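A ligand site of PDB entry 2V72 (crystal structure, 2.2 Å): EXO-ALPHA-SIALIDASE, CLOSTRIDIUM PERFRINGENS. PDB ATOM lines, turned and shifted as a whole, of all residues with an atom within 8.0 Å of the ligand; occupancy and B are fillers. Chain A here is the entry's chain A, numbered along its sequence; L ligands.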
ATOM      1  N   GLU A  24      -6.598 -13.503  22.243  1.00  0.00           N
ATOM      2  CA  GLU A  24      -7.484 -13.536  21.106  1.00  0.00           C
ATOM      3  C   GLU A  24      -6.639 -13.838  19.875  1.00  0.00           C
ATOM      4  O   GLU A  24      -5.527 -13.332  19.766  1.00  0.00           O
ATOM      5  CB  GLU A  24      -8.206 -12.190  20.950  1.00  0.00           C
ATOM      6  CG  GLU A  24      -9.220 -12.130  19.809  1.00  0.00           C
ATOM      7  CD  GLU A  24     -10.314 -13.197  19.906  1.00  0.00           C
ATOM      8  OE1 GLU A  24     -10.860 -13.439  21.008  1.00  0.00           O
ATOM      9  OE2 GLU A  24     -10.626 -13.794  18.855  1.00  0.00           O
ATOM     10  N   GLN A  26      -6.742 -12.854  16.878  1.00  0.00           N
ATOM     11  CA  GLN A  26      -6.406 -11.586  16.221  1.00  0.00           C
ATOM     12  C   GLN A  26      -5.374 -10.764  17.002  1.00  0.00           C
ATOM     13  O   GLN A  26      -4.620  -9.986  16.415  1.00  0.00           O
ATOM     14  CB  GLN A  26      -7.703 -10.783  16.059  1.00  0.00           C
ATOM     15  CG  GLN A  26      -7.561  -9.351  15.625  1.00  0.00           C
ATOM     16  CD  GLN A  26      -8.902  -8.657  15.522  1.00  0.00           C
ATOM     17  OE1 GLN A  26      -9.896  -9.245  15.091  1.00  0.00           O
ATOM     18  NE2 GLN A  26      -8.934  -7.393  15.923  1.00  0.00           N
ATOM     19  N   ASP A  27      -5.345 -10.937  18.329  1.00  0.00           N
ATOM     20  CA  ASP A  27      -4.489 -10.179  19.234  1.00  0.00           C
ATOM     21  C   ASP A  27      -3.503 -11.059  19.993  1.00  0.00           C
ATOM     22  O   ASP A  27      -3.650 -11.235  21.205  1.00  0.00           O
ATOM     23  CB  ASP A  27      -5.355  -9.417  20.241  1.00  0.00           C
ATOM     24  CG  ASP A  27      -6.341  -8.475  19.578  1.00  0.00           C
ATOM     25  OD1 ASP A  27      -6.098  -8.056  18.435  1.00  0.00           O
ATOM     26  OD2 ASP A  27      -7.365  -8.151  20.211  1.00  0.00           O
ATOM     27  N   MET A  40      -2.387  -4.921  19.089  1.00  0.00           N
ATOM     28  CA  MET A  40      -2.286  -5.189  20.534  1.00  0.00           C
ATOM     29  C   MET A  40      -2.306  -6.673  20.894  1.00  0.00           C
ATOM     30  O   MET A  40      -2.793  -7.499  20.117  1.00  0.00           O
ATOM     31  CB  MET A  40      -3.434  -4.497  21.268  1.00  0.00           C
ATOM     32  CG  MET A  40      -4.806  -5.054  20.955  1.00  0.00           C
ATOM     33  SD  MET A  40      -6.087  -4.043  21.696  1.00  0.00           S
ATOM     34  CE  MET A  40      -6.340  -2.859  20.380  1.00  0.00           C
ATOM     35  N   TRP A  41      -1.770  -6.986  22.081  1.00  0.00           N
ATOM     36  CA  TRP A  41      -2.095  -8.220  22.761  1.00  0.00           C
ATOM     37  C   TRP A  41      -3.392  -7.963  23.522  1.00  0.00           C
ATOM     38  O   TRP A  41      -3.567  -6.909  24.114  1.00  0.00           O
ATOM     39  CB  TRP A  41      -0.981  -8.649  23.750  1.00  0.00           C
ATOM     40  CG  TRP A  41      -1.471  -9.685  24.735  1.00  0.00           C
ATOM     41  CD1 TRP A  41      -1.861 -10.965  24.440  1.00  0.00           C
ATOM     42  CD2 TRP A  41      -1.678  -9.517  26.151  1.00  0.00           C
ATOM     43  NE1 TRP A  41      -2.279 -11.601  25.589  1.00  0.00           N
ATOM     44  CE2 TRP A  41      -2.172 -10.752  26.650  1.00  0.00           C
ATOM     45  CE3 TRP A  41      -1.470  -8.453  27.050  1.00  0.00           C
ATOM     46  CZ2 TRP A  41      -2.467 -10.949  27.998  1.00  0.00           C
ATOM     47  CZ3 TRP A  41      -1.761  -8.660  28.388  1.00  0.00           C
ATOM     48  CH2 TRP A  41      -2.256  -9.897  28.857  1.00  0.00           C
ATOM     49  N   HIS A  42      -4.287  -8.944  23.501  1.00  0.00           N
ATOM     50  CA  HIS A  42      -5.571  -8.803  24.154  1.00  0.00           C
ATOM     51  C   HIS A  42      -6.018 -10.213  24.525  1.00  0.00           C
ATOM     52  O   HIS A  42      -5.830 -11.148  23.744  1.00  0.00           O
ATOM     53  CB  HIS A  42      -6.562  -8.138  23.190  1.00  0.00           C
ATOM     54  CG  HIS A  42      -7.818  -7.625  23.825  1.00  0.00           C
ATOM     55  ND1 HIS A  42      -8.686  -8.430  24.525  1.00  0.00           N
ATOM     56  CD2 HIS A  42      -8.391  -6.392  23.807  1.00  0.00           C
ATOM     57  CE1 HIS A  42      -9.723  -7.722  24.931  1.00  0.00           C
ATOM     58  NE2 HIS A  42      -9.571  -6.477  24.503  1.00  0.00           N
ATOM     59  N   THR A  43      -6.570 -10.360  25.730  1.00  0.00           N
ATOM     60  CA  THR A  43      -7.111 -11.647  26.156  1.00  0.00           C
ATOM     61  C   THR A  43      -8.318 -11.975  25.293  1.00  0.00           C
ATOM     62  O   THR A  43      -8.793 -11.114  24.547  1.00  0.00           O
ATOM     63  CB  THR A  43      -7.452 -11.644  27.660  1.00  0.00           C
ATOM     64  OG1 THR A  43      -8.407 -10.619  27.949  1.00  0.00           O
ATOM     65  CG2 THR A  43      -6.180 -11.419  28.508  1.00  0.00           C
ATOM     66  N   LYS A  44      -8.826 -13.202  25.357  1.00  0.00           N
ATOM     67  CA  LYS A  44      -9.869 -13.590  24.405  1.00  0.00           C
ATOM     68  C   LYS A  44     -11.201 -12.882  24.619  1.00  0.00           C
ATOM     69  O   LYS A  44     -11.724 -12.821  25.730  1.00  0.00           O
ATOM     70  CB  LYS A  44     -10.030 -15.111  24.234  1.00  0.00           C
ATOM     71  CG  LYS A  44     -10.231 -15.924  25.479  1.00  0.00           C
ATOM     72  CD  LYS A  44     -10.291 -17.430  25.126  1.00  0.00           C
ATOM     73  CE  LYS A  44      -9.067 -17.907  24.345  1.00  0.00           C
ATOM     74  NZ  LYS A  44      -9.113 -19.370  24.018  1.00  0.00           N
ATOM     75  N   TRP A  45     -11.688 -12.317  23.524  1.00  0.00           N
ATOM     76  CA  TRP A  45     -12.832 -11.419  23.521  1.00  0.00           C
ATOM     77  C   TRP A  45     -14.098 -11.989  24.155  1.00  0.00           C
ATOM     78  O   TRP A  45     -14.909 -11.229  24.683  1.00  0.00           O
ATOM     79  CB  TRP A  45     -13.130 -10.996  22.084  1.00  0.00           C
ATOM     80  CG  TRP A  45     -12.060 -10.182  21.401  1.00  0.00           C
ATOM     81  CD1 TRP A  45     -10.801  -9.877  21.867  1.00  0.00           C
ATOM     82  CD2 TRP A  45     -12.150  -9.597  20.091  1.00  0.00           C
ATOM     83  NE1 TRP A  45     -10.120  -9.127  20.929  1.00  0.00           N
ATOM     84  CE2 TRP A  45     -10.921  -8.951  19.838  1.00  0.00           C
ATOM     85  CE3 TRP A  45     -13.164  -9.558  19.120  1.00  0.00           C
ATOM     86  CZ2 TRP A  45     -10.680  -8.258  18.639  1.00  0.00           C
ATOM     87  CZ3 TRP A  45     -12.911  -8.873  17.933  1.00  0.00           C
ATOM     88  CH2 TRP A  45     -11.675  -8.233  17.701  1.00  0.00           C
ATOM     89  N   ASN A  46     -14.263 -13.315  24.111  1.00  0.00           N
ATOM     90  CA  ASN A  46     -15.458 -13.961  24.664  1.00  0.00           C
ATOM     91  C   ASN A  46     -15.492 -14.047  26.193  1.00  0.00           C
ATOM     92  O   ASN A  46     -16.440 -14.583  26.773  1.00  0.00           O
ATOM     93  CB  ASN A  46     -15.755 -15.331  24.016  1.00  0.00           C
ATOM     94  CG  ASN A  46     -14.694 -16.400  24.324  1.00  0.00           C
ATOM     95  OD1 ASN A  46     -14.633 -17.430  23.646  1.00  0.00           O
ATOM     96  ND2 ASN A  46     -13.857 -16.168  25.333  1.00  0.00           N
ATOM     97  N   GLY A  47     -14.456 -13.494  26.835  1.00  0.00           N
ATOM     98  CA  GLY A  47     -14.392 -13.363  28.282  1.00  0.00           C
ATOM     99  C   GLY A  47     -14.237 -14.660  29.057  1.00  0.00           C
ATOM    100  O   GLY A  47     -14.538 -14.709  30.251  1.00  0.00           O
ATOM    101  N   ARG A  73      -3.970   0.327  24.401  1.00  0.00           N
ATOM    102  CA  ARG A  73      -4.607   0.411  23.096  1.00  0.00           C
ATOM    103  C   ARG A  73      -4.860   1.855  22.667  1.00  0.00           C
ATOM    104  O   ARG A  73      -5.348   2.680  23.440  1.00  0.00           O
ATOM    105  CB  ARG A  73      -5.897  -0.405  23.073  1.00  0.00           C
ATOM    106  CG  ARG A  73      -6.958   0.021  24.072  1.00  0.00           C
ATOM    107  CD  ARG A  73      -8.089  -0.990  24.116  1.00  0.00           C
ATOM    108  NE  ARG A  73      -8.747  -1.130  22.829  1.00  0.00           N
ATOM    109  CZ  ARG A  73      -9.446  -2.197  22.445  1.00  0.00           C
ATOM    110  NH1 ARG A  73      -9.576  -3.261  23.238  1.00  0.00           N
ATOM    111  NH2 ARG A  73      -9.999  -2.218  21.242  1.00  0.00           N
ATOM    112  N   SER A  75      -6.973   3.019  20.744  1.00  0.00           N
ATOM    113  CA  SER A  75      -8.399   3.281  20.577  1.00  0.00           C
ATOM    114  C   SER A  75      -9.186   2.216  21.355  1.00  0.00           C
ATOM    115  O   SER A  75      -8.724   1.089  21.512  1.00  0.00           O
ATOM    116  CB  SER A  75      -8.756   3.239  19.092  1.00  0.00           C
ATOM    117  OG  SER A  75     -10.148   3.198  18.889  1.00  0.00           O
ATOM    118  N   GLY A  76     -10.372   2.584  21.841  1.00  0.00           N
ATOM    119  CA  GLY A  76     -11.168   1.706  22.700  1.00  0.00           C
ATOM    120  C   GLY A  76     -10.629   1.697  24.129  1.00  0.00           C
ATOM    121  O   GLY A  76      -9.532   2.183  24.371  1.00  0.00           O
ATOM    122  N   ASN A  77     -11.399   1.145  25.068  1.00  0.00           N
ATOM    123  CA  ASN A  77     -10.914   1.035  26.448  1.00  0.00           C
ATOM    124  C   ASN A  77     -10.789  -0.388  27.032  1.00  0.00           C
ATOM    125  O   ASN A  77     -10.145  -0.588  28.068  1.00  0.00           O
ATOM    126  CB  ASN A  77     -11.658   1.990  27.398  1.00  0.00           C
ATOM    127  CG  ASN A  77     -13.137   1.659  27.558  1.00  0.00           C
ATOM    128  OD1 ASN A  77     -13.838   2.309  28.340  1.00  0.00           O
ATOM    129  ND2 ASN A  77     -13.620   0.644  26.837  1.00  0.00           N
ATOM    130  N   ASN A  78     -11.392  -1.367  26.359  1.00  0.00           N
ATOM    131  CA  ASN A  78     -11.377  -2.750  26.832  1.00  0.00           C
ATOM    132  C   ASN A  78      -9.967  -3.260  27.105  1.00  0.00           C
ATOM    133  O   ASN A  78      -9.108  -3.235  26.223  1.00  0.00           O
ATOM    134  CB  ASN A  78     -12.081  -3.681  25.832  1.00  0.00           C
ATOM    135  CG  ASN A  78     -13.556  -3.840  26.115  1.00  0.00           C
ATOM    136  OD1 ASN A  78     -14.005  -3.733  27.254  1.00  0.00           O
ATOM    137  ND2 ASN A  78     -14.330  -4.103  25.071  1.00  0.00           N
ATOM    138  N   GLY A  79      -9.749  -3.703  28.337  1.00  0.00           N
ATOM    139  CA  GLY A  79      -8.470  -4.267  28.724  1.00  0.00           C
ATOM    140  C   GLY A  79      -7.436  -3.283  29.246  1.00  0.00           C
ATOM    141  O   GLY A  79      -6.285  -3.662  29.484  1.00  0.00           O
ATOM    142  N   VAL A 130     -10.423  -3.147  32.519  1.00  0.00           N
ATOM    143  CA  VAL A 130     -11.782  -2.799  32.106  1.00  0.00           C
ATOM    144  C   VAL A 130     -12.414  -3.818  31.153  1.00  0.00           C
ATOM    145  O   VAL A 130     -11.753  -4.337  30.241  1.00  0.00           O
ATOM    146  CB  VAL A 130     -11.957  -1.308  31.610  1.00  0.00           C
ATOM    147  CG1 VAL A 130     -10.634  -0.569  31.558  1.00  0.00           C
ATOM    148  CG2 VAL A 130     -12.708  -1.208  30.292  1.00  0.00           C
ATOM    149  N   GLY A 131     -13.686  -4.110  31.418  1.00  0.00           N
ATOM    150  CA  GLY A 131     -14.432  -5.118  30.689  1.00  0.00           C
ATOM    151  C   GLY A 131     -14.092  -6.524  31.160  1.00  0.00           C
ATOM    152  O   GLY A 131     -14.698  -7.494  30.708  1.00  0.00           O
ATOM    153  N   PHE A 133     -10.976  -7.593  30.781  1.00  0.00           N
ATOM    154  CA  PHE A 133      -9.942  -7.964  29.808  1.00  0.00           C
ATOM    155  C   PHE A 133      -8.585  -7.363  30.175  1.00  0.00           C
ATOM    156  O   PHE A 133      -8.469  -6.566  31.093  1.00  0.00           O
ATOM    157  CB  PHE A 133     -10.320  -7.512  28.391  1.00  0.00           C
ATOM    158  CG  PHE A 133     -11.672  -7.985  27.939  1.00  0.00           C
ATOM    159  CD1 PHE A 133     -12.750  -7.113  27.918  1.00  0.00           C
ATOM    160  CD2 PHE A 133     -11.862  -9.299  27.534  1.00  0.00           C
ATOM    161  CE1 PHE A 133     -14.009  -7.548  27.500  1.00  0.00           C
ATOM    162  CE2 PHE A 133     -13.110  -9.751  27.127  1.00  0.00           C
ATOM    163  CZ  PHE A 133     -14.185  -8.869  27.108  1.00  0.00           C
ATOM    164  N   ALA A 134      -7.559  -7.765  29.421  1.00  0.00           N
ATOM    165  CA  ALA A 134      -6.242  -7.164  29.495  1.00  0.00           C
ATOM    166  C   ALA A 134      -5.770  -6.954  28.055  1.00  0.00           C
ATOM    167  O   ALA A 134      -5.865  -7.868  27.232  1.00  0.00           O
ATOM    168  CB  ALA A 134      -5.274  -8.077  30.238  1.00  0.00           C
ATOM    169  N   SER A 135      -5.282  -5.742  27.776  1.00  0.00           N
ATOM    170  CA  SER A 135      -4.681  -5.415  26.485  1.00  0.00           C
ATOM    171  C   SER A 135      -3.430  -4.552  26.664  1.00  0.00           C
ATOM    172  O   SER A 135      -3.329  -3.753  27.596  1.00  0.00           O
ATOM    173  CB  SER A 135      -5.687  -4.731  25.546  1.00  0.00           C
ATOM    174  OG  SER A 135      -6.260  -3.569  26.108  1.00  0.00           O
HETATM  175  C1  LIG L   1     -14.316  -4.996  20.887  1.00  0.00           C
HETATM  176  C2  LIG L   1     -12.890  -4.435  20.860  1.00  0.00           C
HETATM  177  C3  LIG L   1     -11.862  -5.568  20.999  1.00  0.00           C
HETATM  178  C4  LIG L   1     -12.206  -6.526  22.138  1.00  0.00           C
HETATM  179  C5  LIG L   1     -13.671  -6.961  22.092  1.00  0.00           C
HETATM  180  C6  LIG L   1     -14.013  -7.799  23.311  1.00  0.00           C
HETATM  181  O1  LIG L   1     -15.211  -3.911  20.953  1.00  0.00           O
HETATM  182  O2  LIG L   1     -12.679  -3.696  19.685  1.00  0.00           O
HETATM  183  O3  LIG L   1     -10.602  -5.007  21.258  1.00  0.00           O
HETATM  184  O4  LIG L   1     -11.960  -5.907  23.389  1.00  0.00           O
HETATM  185  O5  LIG L   1     -14.515  -5.814  22.021  1.00  0.00           O
HETATM  186  O6  LIG L   1     -15.233  -8.477  23.083  1.00  0.00           O
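The backbone carbonyl oxygen (O) of Asn 78 sits at hydrogen-bond distance from the side-chain hydroxyl (OG) of Ser 135 (2.9 Å).
NH1 of Arg 73 sits at hydrogen-bond distance from O of Asn 78 (3.0 Å).
A ring nitrogen (NE2) of His 42 lies close to the guanidinium group (NH1) of Arg 73.
The backbone NH of Trp 45 sits at hydrogen-bond distance from the side-chain carboxylate of Glu 24.
The guanidinium group (NE) of Arg 73 is in hydrogen-bond range of the backbone carbonyl oxygen (O) of Ser 75, at 2.6 Å.
The indole nitrogen of Trp 45 sits at hydrogen-bond distance from the side-chain carboxylate of Asp 27 (3.0 Å).
The backbone carbonyl oxygen of His 42 sits at hydrogen-bond distance from the backbone NH of Glu 24, 2.9 Å away.
The backbone carbonyl oxygen (O) of Asp 27 sits at hydrogen-bond distance from the backbone NH (N) of His 42 (3.3 Å).
O of Trp 45 sits at hydrogen-bond distance from O6 of the ligand (3.2 Å).
NH1 of Arg 73 lies within hydrogen-bond range of O3 of the ligand (2.8 Å).
O4 of the ligand lies close to ND2 of Asn 78 (3.4 Å).
A ring nitrogen (NE2) of His 42 lies within hydrogen-bond range of an oxygen (O4) of the ligand (2.7 Å).
Residues that only touch the ligand: Phe 133 (3.9 Å).
Within 4 Å of the ligand: His 42, Trp 45, Arg 73, Asn 78 and Phe 133.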
